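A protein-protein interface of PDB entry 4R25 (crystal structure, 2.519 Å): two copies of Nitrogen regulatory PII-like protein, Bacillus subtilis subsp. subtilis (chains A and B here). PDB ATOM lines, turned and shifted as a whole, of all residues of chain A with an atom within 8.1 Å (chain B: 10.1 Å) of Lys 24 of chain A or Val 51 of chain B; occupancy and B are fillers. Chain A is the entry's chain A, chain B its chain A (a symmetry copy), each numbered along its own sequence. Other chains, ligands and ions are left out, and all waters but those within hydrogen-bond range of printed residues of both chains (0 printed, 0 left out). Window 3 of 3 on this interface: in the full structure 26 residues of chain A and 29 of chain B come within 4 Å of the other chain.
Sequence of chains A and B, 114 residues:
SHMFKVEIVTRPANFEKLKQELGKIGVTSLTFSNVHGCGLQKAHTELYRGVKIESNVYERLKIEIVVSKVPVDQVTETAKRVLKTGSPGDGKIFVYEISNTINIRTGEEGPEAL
The backbone NH (N) of Leu 40 of chain B is in hydrogen-bond range of the backbone carbonyl oxygen (O) of Thr 28 of chain A, at 2.8 Å.
The side-chain amide nitrogen (NE2) of Gln 20 of chain A is in hydrogen-bond range of the backbone carbonyl oxygen (O) of Ile 53 of chain B (3.1 Å).
The backbone carbonyl oxygen of Leu 22 of chain A lies within hydrogen-bond range of the backbone NH of Val 27 of chain A (3.1 Å).
The side-chain carboxylate of Glu 21 of chain A lies within salt-bridge range of the side-chain amino group of Lys 24 of chain A, at 3.9 Å.
Among the printed residues, pairs that only touch across the chains: Lys 19 of chain A with Leu 40 of chain B (3.7 Å), Lys 19 of chain A with Ile 53 of chain B (3.9 Å), Gly 23 of chain A with Leu 40 of chain B (3.8 Å), Gly 23 of chain A with Lys 42 of chain B (3.8 Å), Gly 23 of chain A with Ile 53 of chain B (3.5 Å), Lys 24 of chain A with Lys 42 of chain B (3.6 Å), Lys 24 of chain A with Val 51 of chain B (3.7 Å), Lys 24 of chain A with Ile 53 of chain B (3.8 Å) and Val 27 of chain A with Leu 40 of chain B (3.4 Å).
No residue of chain B comes within 4 Å of Ile 25 of chain A.
Of the printed residues of chain B, Thr 28 of chain A touches Leu 40.
Of the printed residues of chain A, Lys 42 of chain B touches Gly 23 and Lys 24.
No residue of chain A comes within 4 Å of Gly 50 of chain B.
Printed residues of chain A within 4 Å of Val 51 of chain B: Lys 24 (3.7 Å).
The nearest residue of chain B that does not touch Lys 24 of chain A is Lys 52 of chain B (4.7 Å).
The nearest residue of chain A that does not touch Val 51 of chain B is Gln 20 of chain A (5.2 Å).
Of the 16 printed residues of chain A, 6 touch a printed residue of chain B.
Of the 15 printed residues of chain B, 4 touch a printed residue of chain A.
Printed residues of chain B that touch a printed residue of chain A: Leu 40, Lys 42, Val 51 and Ile 53.
Hydrophobic or aromatic side chains of chain B within 4 Å of the printed part of chain A: Leu 40 and Ile 53.
No position is printed for both chains.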
ATOM      1  N   LYS A  17     -36.235 -22.954  25.709  1.00  0.00           N
ATOM      2  CA  LYS A  17     -35.460 -21.841  26.250  1.00  0.00           C
ATOM      3  C   LYS A  17     -33.980 -22.214  26.300  1.00  0.00           C
ATOM      4  O   LYS A  17     -33.111 -21.353  26.138  1.00  0.00           O
ATOM      5  CB  LYS A  17     -35.967 -21.434  27.643  1.00  0.00           C
ATOM      6  CG  LYS A  17     -35.326 -20.153  28.210  1.00  0.00           C
ATOM      7  CD  LYS A  17     -36.091 -19.621  29.438  1.00  0.00           C
ATOM      8  CE  LYS A  17     -35.252 -18.663  30.303  1.00  0.00           C
ATOM      9  NZ  LYS A  17     -34.716 -17.484  29.562  1.00  0.00           N
ATOM     10  N   LEU A  18     -33.698 -23.499  26.514  1.00  0.00           N
ATOM     11  CA  LEU A  18     -32.323 -23.978  26.583  1.00  0.00           C
ATOM     12  C   LEU A  18     -31.634 -23.828  25.228  1.00  0.00           C
ATOM     13  O   LEU A  18     -30.522 -23.305  25.136  1.00  0.00           O
ATOM     14  CB  LEU A  18     -32.301 -25.442  27.018  1.00  0.00           C
ATOM     15  CG  LEU A  18     -31.327 -25.938  28.090  1.00  0.00           C
ATOM     16  CD1 LEU A  18     -30.916 -27.366  27.770  1.00  0.00           C
ATOM     17  CD2 LEU A  18     -30.093 -25.058  28.222  1.00  0.00           C
ATOM     18  N   LYS A  19     -32.296 -24.306  24.182  1.00  0.00           N
ATOM     19  CA  LYS A  19     -31.779 -24.179  22.829  1.00  0.00           C
ATOM     20  C   LYS A  19     -31.500 -22.716  22.487  1.00  0.00           C
ATOM     21  O   LYS A  19     -30.476 -22.411  21.874  1.00  0.00           O
ATOM     22  CB  LYS A  19     -32.748 -24.795  21.822  1.00  0.00           C
ATOM     23  CG  LYS A  19     -32.991 -26.277  22.027  1.00  0.00           C
ATOM     24  CD  LYS A  19     -34.008 -26.803  21.038  1.00  0.00           C
ATOM     25  CE  LYS A  19     -34.301 -28.271  21.257  1.00  0.00           C
ATOM     26  NZ  LYS A  19     -35.325 -28.741  20.281  1.00  0.00           N
ATOM     27  N   GLN A  20     -32.402 -21.816  22.888  1.00  0.00           N
ATOM     28  CA  GLN A  20     -32.184 -20.379  22.688  1.00  0.00           C
ATOM     29  C   GLN A  20     -30.924 -19.906  23.389  1.00  0.00           C
ATOM     30  O   GLN A  20     -30.076 -19.239  22.787  1.00  0.00           O
ATOM     31  CB  GLN A  20     -33.372 -19.538  23.181  1.00  0.00           C
ATOM     32  CG  GLN A  20     -34.650 -19.672  22.354  1.00  0.00           C
ATOM     33  CD  GLN A  20     -34.465 -19.268  20.898  1.00  0.00           C
ATOM     34  OE1 GLN A  20     -33.960 -18.183  20.595  1.00  0.00           O
ATOM     35  NE2 GLN A  20     -34.885 -20.140  19.988  1.00  0.00           N
ATOM     36  N   GLU A  21     -30.800 -20.252  24.666  1.00  0.00           N
ATOM     37  CA  GLU A  21     -29.689 -19.745  25.465  1.00  0.00           C
ATOM     38  C   GLU A  21     -28.355 -20.371  25.068  1.00  0.00           C
ATOM     39  O   GLU A  21     -27.339 -19.682  24.993  1.00  0.00           O
ATOM     40  CB  GLU A  21     -29.967 -19.937  26.957  1.00  0.00           C
ATOM     41  CG  GLU A  21     -31.264 -19.286  27.435  1.00  0.00           C
ATOM     42  CD  GLU A  21     -31.257 -17.769  27.303  1.00  0.00           C
ATOM     43  OE1 GLU A  21     -30.677 -17.097  28.183  1.00  0.00           O
ATOM     44  OE2 GLU A  21     -31.838 -17.247  26.324  1.00  0.00           O
ATOM     45  N   LEU A  22     -28.354 -21.674  24.806  1.00  0.00           N
ATOM     46  CA  LEU A  22     -27.124 -22.341  24.404  1.00  0.00           C
ATOM     47  C   LEU A  22     -26.705 -21.836  23.034  1.00  0.00           C
ATOM     48  O   LEU A  22     -25.525 -21.569  22.792  1.00  0.00           O
ATOM     49  CB  LEU A  22     -27.295 -23.863  24.388  1.00  0.00           C
ATOM     50  CG  LEU A  22     -27.480 -24.508  25.760  1.00  0.00           C
ATOM     51  CD1 LEU A  22     -27.789 -25.982  25.606  1.00  0.00           C
ATOM     52  CD2 LEU A  22     -26.245 -24.287  26.621  1.00  0.00           C
ATOM     53  N   GLY A  23     -27.680 -21.710  22.142  1.00  0.00           N
ATOM     54  CA  GLY A  23     -27.442 -21.120  20.835  1.00  0.00           C
ATOM     55  C   GLY A  23     -26.741 -19.767  20.909  1.00  0.00           C
ATOM     56  O   GLY A  23     -25.809 -19.503  20.149  1.00  0.00           O
ATOM     57  N   LYS A  24     -27.164 -18.916  21.844  1.00  0.00           N
ATOM     58  CA  LYS A  24     -26.646 -17.549  21.895  1.00  0.00           C
ATOM     59  C   LYS A  24     -25.205 -17.464  22.340  1.00  0.00           C
ATOM     60  O   LYS A  24     -24.491 -16.552  21.930  1.00  0.00           O
ATOM     61  CB  LYS A  24     -27.538 -16.646  22.748  1.00  0.00           C
ATOM     62  CG  LYS A  24     -28.807 -16.242  22.018  1.00  0.00           C
ATOM     63  CD  LYS A  24     -29.902 -15.756  22.957  1.00  0.00           C
ATOM     64  CE  LYS A  24     -31.213 -15.612  22.175  1.00  0.00           C
ATOM     65  NZ  LYS A  24     -32.401 -15.295  23.014  1.00  0.00           N
ATOM     66  N   ILE A  25     -24.770 -18.413  23.163  1.00  0.00           N
ATOM     67  CA  ILE A  25     -23.398 -18.389  23.676  1.00  0.00           C
ATOM     68  C   ILE A  25     -22.410 -19.126  22.763  1.00  0.00           C
ATOM     69  O   ILE A  25     -21.216 -19.181  23.049  1.00  0.00           O
ATOM     70  CB  ILE A  25     -23.308 -18.961  25.101  1.00  0.00           C
ATOM     71  CG1 ILE A  25     -23.198 -20.492  25.071  1.00  0.00           C
ATOM     72  CG2 ILE A  25     -24.517 -18.525  25.910  1.00  0.00           C
ATOM     73  CD1 ILE A  25     -23.302 -21.153  26.428  1.00  0.00           C
ATOM     74  N   GLY A  26     -22.903 -19.692  21.665  1.00  0.00           N
ATOM     75  CA  GLY A  26     -22.013 -20.297  20.688  1.00  0.00           C
ATOM     76  C   GLY A  26     -22.241 -21.750  20.294  1.00  0.00           C
ATOM     77  O   GLY A  26     -21.646 -22.211  19.322  1.00  0.00           O
ATOM     78  N   VAL A  27     -23.083 -22.479  21.027  1.00  0.00           N
ATOM     79  CA  VAL A  27     -23.336 -23.878  20.687  1.00  0.00           C
ATOM     80  C   VAL A  27     -24.111 -24.007  19.380  1.00  0.00           C
ATOM     81  O   VAL A  27     -25.166 -23.390  19.214  1.00  0.00           O
ATOM     82  CB  VAL A  27     -24.110 -24.620  21.782  1.00  0.00           C
ATOM     83  CG1 VAL A  27     -24.331 -26.060  21.362  1.00  0.00           C
ATOM     84  CG2 VAL A  27     -23.367 -24.544  23.108  1.00  0.00           C
ATOM     85  N   THR A  28     -23.592 -24.819  18.460  1.00  0.00           N
ATOM     86  CA  THR A  28     -24.231 -25.002  17.156  1.00  0.00           C
ATOM     87  C   THR A  28     -24.833 -26.395  16.940  1.00  0.00           C
ATOM     88  O   THR A  28     -25.531 -26.625  15.958  1.00  0.00           O
ATOM     89  CB  THR A  28     -23.265 -24.682  16.006  1.00  0.00           C
ATOM     90  OG1 THR A  28     -22.245 -25.685  15.940  1.00  0.00           O
ATOM     91  CG2 THR A  28     -22.613 -23.326  16.224  1.00  0.00           C
ATOM     92  N   VAL A  70     -16.193 -22.580  22.864  1.00  0.00           N
ATOM     93  CA  VAL A  70     -17.199 -22.194  23.838  1.00  0.00           C
ATOM     94  C   VAL A  70     -16.871 -22.826  25.176  1.00  0.00           C
ATOM     95  O   VAL A  70     -16.785 -24.049  25.286  1.00  0.00           O
ATOM     96  CB  VAL A  70     -18.582 -22.668  23.432  1.00  0.00           C
ATOM     97  CG1 VAL A  70     -19.581 -22.303  24.513  1.00  0.00           C
ATOM     98  CG2 VAL A  70     -18.964 -22.079  22.076  1.00  0.00           C
ATOM     99  N   GLN A  74     -19.464 -21.481  30.815  1.00  0.00           N
ATOM    100  CA  GLN A  74     -20.549 -20.692  30.248  1.00  0.00           C
ATOM    101  C   GLN A  74     -21.704 -21.621  29.855  1.00  0.00           C
ATOM    102  O   GLN A  74     -22.865 -21.238  29.955  1.00  0.00           O
ATOM    103  CB  GLN A  74     -20.054 -19.878  29.043  1.00  0.00           C
ATOM    104  CG  GLN A  74     -20.829 -18.583  28.782  1.00  0.00           C
ATOM    105  CD  GLN A  74     -20.239 -17.731  27.653  1.00  0.00           C
ATOM    106  OE1 GLN A  74     -20.952 -16.965  26.997  1.00  0.00           O
ATOM    107  NE2 GLN A  74     -18.937 -17.864  27.429  1.00  0.00           N
ATOM    108  N   THR A  78     -25.273 -21.427  32.142  1.00  0.00           N
ATOM    109  CA  THR A  78     -26.486 -21.166  31.389  1.00  0.00           C
ATOM    110  C   THR A  78     -27.498 -22.270  31.625  1.00  0.00           C
ATOM    111  O   THR A  78     -28.688 -22.014  31.758  1.00  0.00           O
ATOM    112  CB  THR A  78     -26.184 -21.082  29.891  1.00  0.00           C
ATOM    113  OG1 THR A  78     -25.136 -20.136  29.679  1.00  0.00           O
ATOM    114  CG2 THR A  78     -27.421 -20.656  29.105  1.00  0.00           C
ATOM    115  N   ARG A  81     -29.216 -21.688  35.232  1.00  0.00           N
ATOM    116  CA  ARG A  81     -30.227 -20.641  35.186  1.00  0.00           C
ATOM    117  C   ARG A  81     -31.515 -21.138  34.573  1.00  0.00           C
ATOM    118  O   ARG A  81     -32.583 -21.044  35.174  1.00  0.00           O
ATOM    119  CB  ARG A  81     -29.744 -19.473  34.340  1.00  0.00           C
ATOM    120  CG  ARG A  81     -28.710 -18.598  34.977  1.00  0.00           C
ATOM    121  CD  ARG A  81     -28.327 -17.521  33.988  1.00  0.00           C
ATOM    122  NE  ARG A  81     -29.376 -17.345  32.987  1.00  0.00           N
ATOM    123  CZ  ARG A  81     -29.151 -17.288  31.679  1.00  0.00           C
ATOM    124  NH1 ARG A  81     -27.911 -17.391  31.223  1.00  0.00           N
ATOM    125  NH2 ARG A  81     -30.159 -17.122  30.830  1.00  0.00           N
ATOM    126  N   LEU B  40     -28.144 -25.757  15.811  1.00  0.00           N
ATOM    127  CA  LEU B  40     -28.497 -24.437  16.305  1.00  0.00           C
ATOM    128  C   LEU B  40     -27.762 -23.361  15.498  1.00  0.00           C
ATOM    129  O   LEU B  40     -26.549 -23.432  15.304  1.00  0.00           O
ATOM    130  CB  LEU B  40     -28.160 -24.309  17.797  1.00  0.00           C
ATOM    131  CG  LEU B  40     -28.767 -25.301  18.796  1.00  0.00           C
ATOM    132  CD1 LEU B  40     -28.393 -24.915  20.208  1.00  0.00           C
ATOM    133  CD2 LEU B  40     -30.269 -25.385  18.676  1.00  0.00           C
ATOM    134  N   GLN B  41     -28.502 -22.369  15.016  1.00  0.00           N
ATOM    135  CA  GLN B  41     -27.873 -21.260  14.307  1.00  0.00           C
ATOM    136  C   GLN B  41     -28.474 -19.898  14.647  1.00  0.00           C
ATOM    137  O   GLN B  41     -29.693 -19.748  14.768  1.00  0.00           O
ATOM    138  CB  GLN B  41     -27.868 -21.502  12.798  1.00  0.00           C
ATOM    139  CG  GLN B  41     -29.033 -22.323  12.301  1.00  0.00           C
ATOM    140  CD  GLN B  41     -28.944 -22.621  10.818  1.00  0.00           C
ATOM    141  OE1 GLN B  41     -27.856 -22.605  10.231  1.00  0.00           O
ATOM    142  NE2 GLN B  41     -30.093 -22.892  10.198  1.00  0.00           N
ATOM    143  N   LYS B  42     -27.581 -18.928  14.832  1.00  0.00           N
ATOM    144  CA  LYS B  42     -27.937 -17.542  15.090  1.00  0.00           C
ATOM    145  C   LYS B  42     -28.629 -16.937  13.887  1.00  0.00           C
ATOM    146  O   LYS B  42     -28.094 -16.939  12.779  1.00  0.00           O
ATOM    147  CB  LYS B  42     -26.689 -16.726  15.417  1.00  0.00           C
ATOM    148  CG  LYS B  42     -26.077 -17.052  16.763  1.00  0.00           C
ATOM    149  CD  LYS B  42     -24.727 -16.378  16.924  1.00  0.00           C
ATOM    150  CE  LYS B  42     -24.145 -16.631  18.309  1.00  0.00           C
ATOM    151  NZ  LYS B  42     -22.726 -16.180  18.406  1.00  0.00           N
ATOM    152  N   ALA B  43     -29.832 -16.436  14.118  1.00  0.00           N
ATOM    153  CA  ALA B  43     -30.608 -15.772  13.088  1.00  0.00           C
ATOM    154  C   ALA B  43     -30.827 -14.307  13.463  1.00  0.00           C
ATOM    155  O   ALA B  43     -30.739 -13.933  14.635  1.00  0.00           O
ATOM    156  CB  ALA B  43     -31.930 -16.482  12.900  1.00  0.00           C
ATOM    157  N   HIS B  44     -31.097 -13.470  12.469  1.00  0.00           N
ATOM    158  CA  HIS B  44     -31.417 -12.076  12.750  1.00  0.00           C
ATOM    159  C   HIS B  44     -32.828 -11.930  13.284  1.00  0.00           C
ATOM    160  O   HIS B  44     -33.749 -12.617  12.845  1.00  0.00           O
ATOM    161  CB  HIS B  44     -31.268 -11.206  11.504  1.00  0.00           C
ATOM    162  CG  HIS B  44     -29.853 -10.842  11.197  1.00  0.00           C
ATOM    163  ND1 HIS B  44     -29.119  -9.987  11.988  1.00  0.00           N
ATOM    164  CD2 HIS B  44     -29.031 -11.226  10.195  1.00  0.00           C
ATOM    165  CE1 HIS B  44     -27.903  -9.854  11.487  1.00  0.00           C
ATOM    166  NE2 HIS B  44     -27.826 -10.599  10.397  1.00  0.00           N
ATOM    167  N   THR B  45     -32.987 -11.036  14.252  1.00  0.00           N
ATOM    168  CA  THR B  45     -34.304 -10.496  14.534  1.00  0.00           C
ATOM    169  C   THR B  45     -34.415  -9.178  13.777  1.00  0.00           C
ATOM    170  O   THR B  45     -33.488  -8.754  13.075  1.00  0.00           O
ATOM    171  CB  THR B  45     -34.556 -10.288  16.047  1.00  0.00           C
ATOM    172  OG1 THR B  45     -33.637  -9.322  16.568  1.00  0.00           O
ATOM    173  CG2 THR B  45     -34.393 -11.602  16.810  1.00  0.00           C
ATOM    174  N   GLU B  46     -35.553  -8.524  13.910  1.00  0.00           N
ATOM    175  CA  GLU B  46     -35.779  -7.278  13.205  1.00  0.00           C
ATOM    176  C   GLU B  46     -34.954  -6.137  13.792  1.00  0.00           C
ATOM    177  O   GLU B  46     -34.559  -5.214  13.082  1.00  0.00           O
ATOM    178  CB  GLU B  46     -37.255  -6.935  13.267  1.00  0.00           C
ATOM    179  CG  GLU B  46     -37.658  -5.838  12.348  1.00  0.00           C
ATOM    180  CD  GLU B  46     -39.122  -5.593  12.447  1.00  0.00           C
ATOM    181  OE1 GLU B  46     -39.705  -6.044  13.452  1.00  0.00           O
ATOM    182  OE2 GLU B  46     -39.689  -4.967  11.530  1.00  0.00           O
ATOM    183  N   LEU B  47     -34.694  -6.204  15.091  1.00  0.00           N
ATOM    184  CA  LEU B  47     -33.941  -5.154  15.765  1.00  0.00           C
ATOM    185  C   LEU B  47     -32.440  -5.401  15.694  1.00  0.00           C
ATOM    186  O   LEU B  47     -31.995  -6.542  15.639  1.00  0.00           O
ATOM    187  CB  LEU B  47     -34.408  -5.022  17.215  1.00  0.00           C
ATOM    188  CG  LEU B  47     -35.925  -4.872  17.326  1.00  0.00           C
ATOM    189  CD1 LEU B  47     -36.371  -4.936  18.770  1.00  0.00           C
ATOM    190  CD2 LEU B  47     -36.400  -3.579  16.664  1.00  0.00           C
ATOM    191  N   TYR B  48     -31.670  -4.320  15.695  1.00  0.00           N
ATOM    192  CA  TYR B  48     -30.218  -4.405  15.598  1.00  0.00           C
ATOM    193  C   TYR B  48     -29.556  -5.205  16.721  1.00  0.00           C
ATOM    194  O   TYR B  48     -28.505  -5.808  16.513  1.00  0.00           O
ATOM    195  CB  TYR B  48     -29.604  -3.004  15.507  1.00  0.00           C
ATOM    196  CG  TYR B  48     -29.062  -2.689  14.138  1.00  0.00           C
ATOM    197  CD1 TYR B  48     -27.725  -2.880  13.842  1.00  0.00           C
ATOM    198  CD2 TYR B  48     -29.892  -2.224  13.137  1.00  0.00           C
ATOM    199  CE1 TYR B  48     -27.228  -2.599  12.582  1.00  0.00           C
ATOM    200  CE2 TYR B  48     -29.410  -1.943  11.886  1.00  0.00           C
ATOM    201  CZ  TYR B  48     -28.082  -2.129  11.608  1.00  0.00           C
ATOM    202  OH  TYR B  48     -27.641  -1.834  10.341  1.00  0.00           O
ATOM    203  N   ARG B  49     -30.162  -5.218  17.902  1.00  0.00           N
ATOM    204  CA  ARG B  49     -29.596  -5.970  19.025  1.00  0.00           C
ATOM    205  C   ARG B  49     -29.889  -7.475  18.972  1.00  0.00           C
ATOM    206  O   ARG B  49     -29.121  -8.299  19.477  1.00  0.00           O
ATOM    207  CB  ARG B  49     -30.145  -5.404  20.336  1.00  0.00           C
ATOM    208  CG  ARG B  49     -31.651  -5.150  20.323  1.00  0.00           C
ATOM    209  CD  ARG B  49     -32.446  -6.318  20.897  1.00  0.00           C
ATOM    210  NE  ARG B  49     -33.105  -7.112  19.862  1.00  0.00           N
ATOM    211  CZ  ARG B  49     -34.319  -7.644  19.985  1.00  0.00           C
ATOM    212  NH1 ARG B  49     -35.016  -7.457  21.097  1.00  0.00           N
ATOM    213  NH2 ARG B  49     -34.840  -8.357  18.990  1.00  0.00           N
ATOM    214  N   GLY B  50     -31.006  -7.819  18.349  1.00  0.00           N
ATOM    215  CA  GLY B  50     -31.627  -9.106  18.554  1.00  0.00           C
ATOM    216  C   GLY B  50     -31.012 -10.312  17.896  1.00  0.00           C
ATOM    217  O   GLY B  50     -30.822 -10.359  16.679  1.00  0.00           O
ATOM    218  N   VAL B  51     -30.702 -11.301  18.723  1.00  0.00           N
ATOM    219  CA  VAL B  51     -30.424 -12.630  18.219  1.00  0.00           C
ATOM    220  C   VAL B  51     -31.626 -13.524  18.499  1.00  0.00           C
ATOM    221  O   VAL B  51     -32.357 -13.343  19.474  1.00  0.00           O
ATOM    222  CB  VAL B  51     -29.130 -13.230  18.790  1.00  0.00           C
ATOM    223  CG1 VAL B  51     -28.901 -14.614  18.219  1.00  0.00           C
ATOM    224  CG2 VAL B  51     -27.942 -12.336  18.446  1.00  0.00           C
ATOM    225  N   LYS B  52     -31.821 -14.484  17.609  1.00  0.00           N
ATOM    226  CA  LYS B  52     -32.897 -15.453  17.709  1.00  0.00           C
ATOM    227  C   LYS B  52     -32.272 -16.744  17.209  1.00  0.00           C
ATOM    228  O   LYS B  52     -31.437 -16.702  16.298  1.00  0.00           O
ATOM    229  CB  LYS B  52     -34.043 -15.016  16.800  1.00  0.00           C
ATOM    230  CG  LYS B  52     -34.929 -16.131  16.287  1.00  0.00           C
ATOM    231  CD  LYS B  52     -34.985 -16.169  14.746  1.00  0.00           C
ATOM    232  CE  LYS B  52     -35.822 -15.047  14.124  1.00  0.00           C
ATOM    233  NZ  LYS B  52     -36.503 -15.445  12.846  1.00  0.00           N
ATOM    234  N   ILE B  53     -32.614 -17.881  17.811  1.00  0.00           N
ATOM    235  CA  ILE B  53     -31.967 -19.135  17.425  1.00  0.00           C
ATOM    236  C   ILE B  53     -32.913 -20.031  16.646  1.00  0.00           C
ATOM    237  O   ILE B  53     -34.049 -20.250  17.046  1.00  0.00           O
ATOM    238  CB  ILE B  53     -31.428 -19.900  18.645  1.00  0.00           C
ATOM    239  CG1 ILE B  53     -30.453 -19.024  19.439  1.00  0.00           C
ATOM    240  CG2 ILE B  53     -30.759 -21.203  18.223  1.00  0.00           C
ATOM    241  CD1 ILE B  53     -29.200 -18.663  18.693  1.00  0.00           C
ATOM    242  N   GLU B  54     -32.434 -20.549  15.525  1.00  0.00           N
ATOM    243  CA  GLU B  54     -33.222 -21.467  14.727  1.00  0.00           C
ATOM    244  C   GLU B  54     -32.603 -22.852  14.853  1.00  0.00           C
ATOM    245  O   GLU B  54     -31.379 -22.995  14.914  1.00  0.00           O
ATOM    246  CB  GLU B  54     -33.237 -21.004  13.279  1.00  0.00           C
ATOM    247  CG  GLU B  54     -34.195 -21.744  12.382  1.00  0.00           C
ATOM    248  CD  GLU B  54     -34.223 -21.135  10.999  1.00  0.00           C
ATOM    249  OE1 GLU B  54     -34.890 -21.697  10.102  1.00  0.00           O
ATOM    250  OE2 GLU B  54     -33.566 -20.085  10.817  1.00  0.00           O
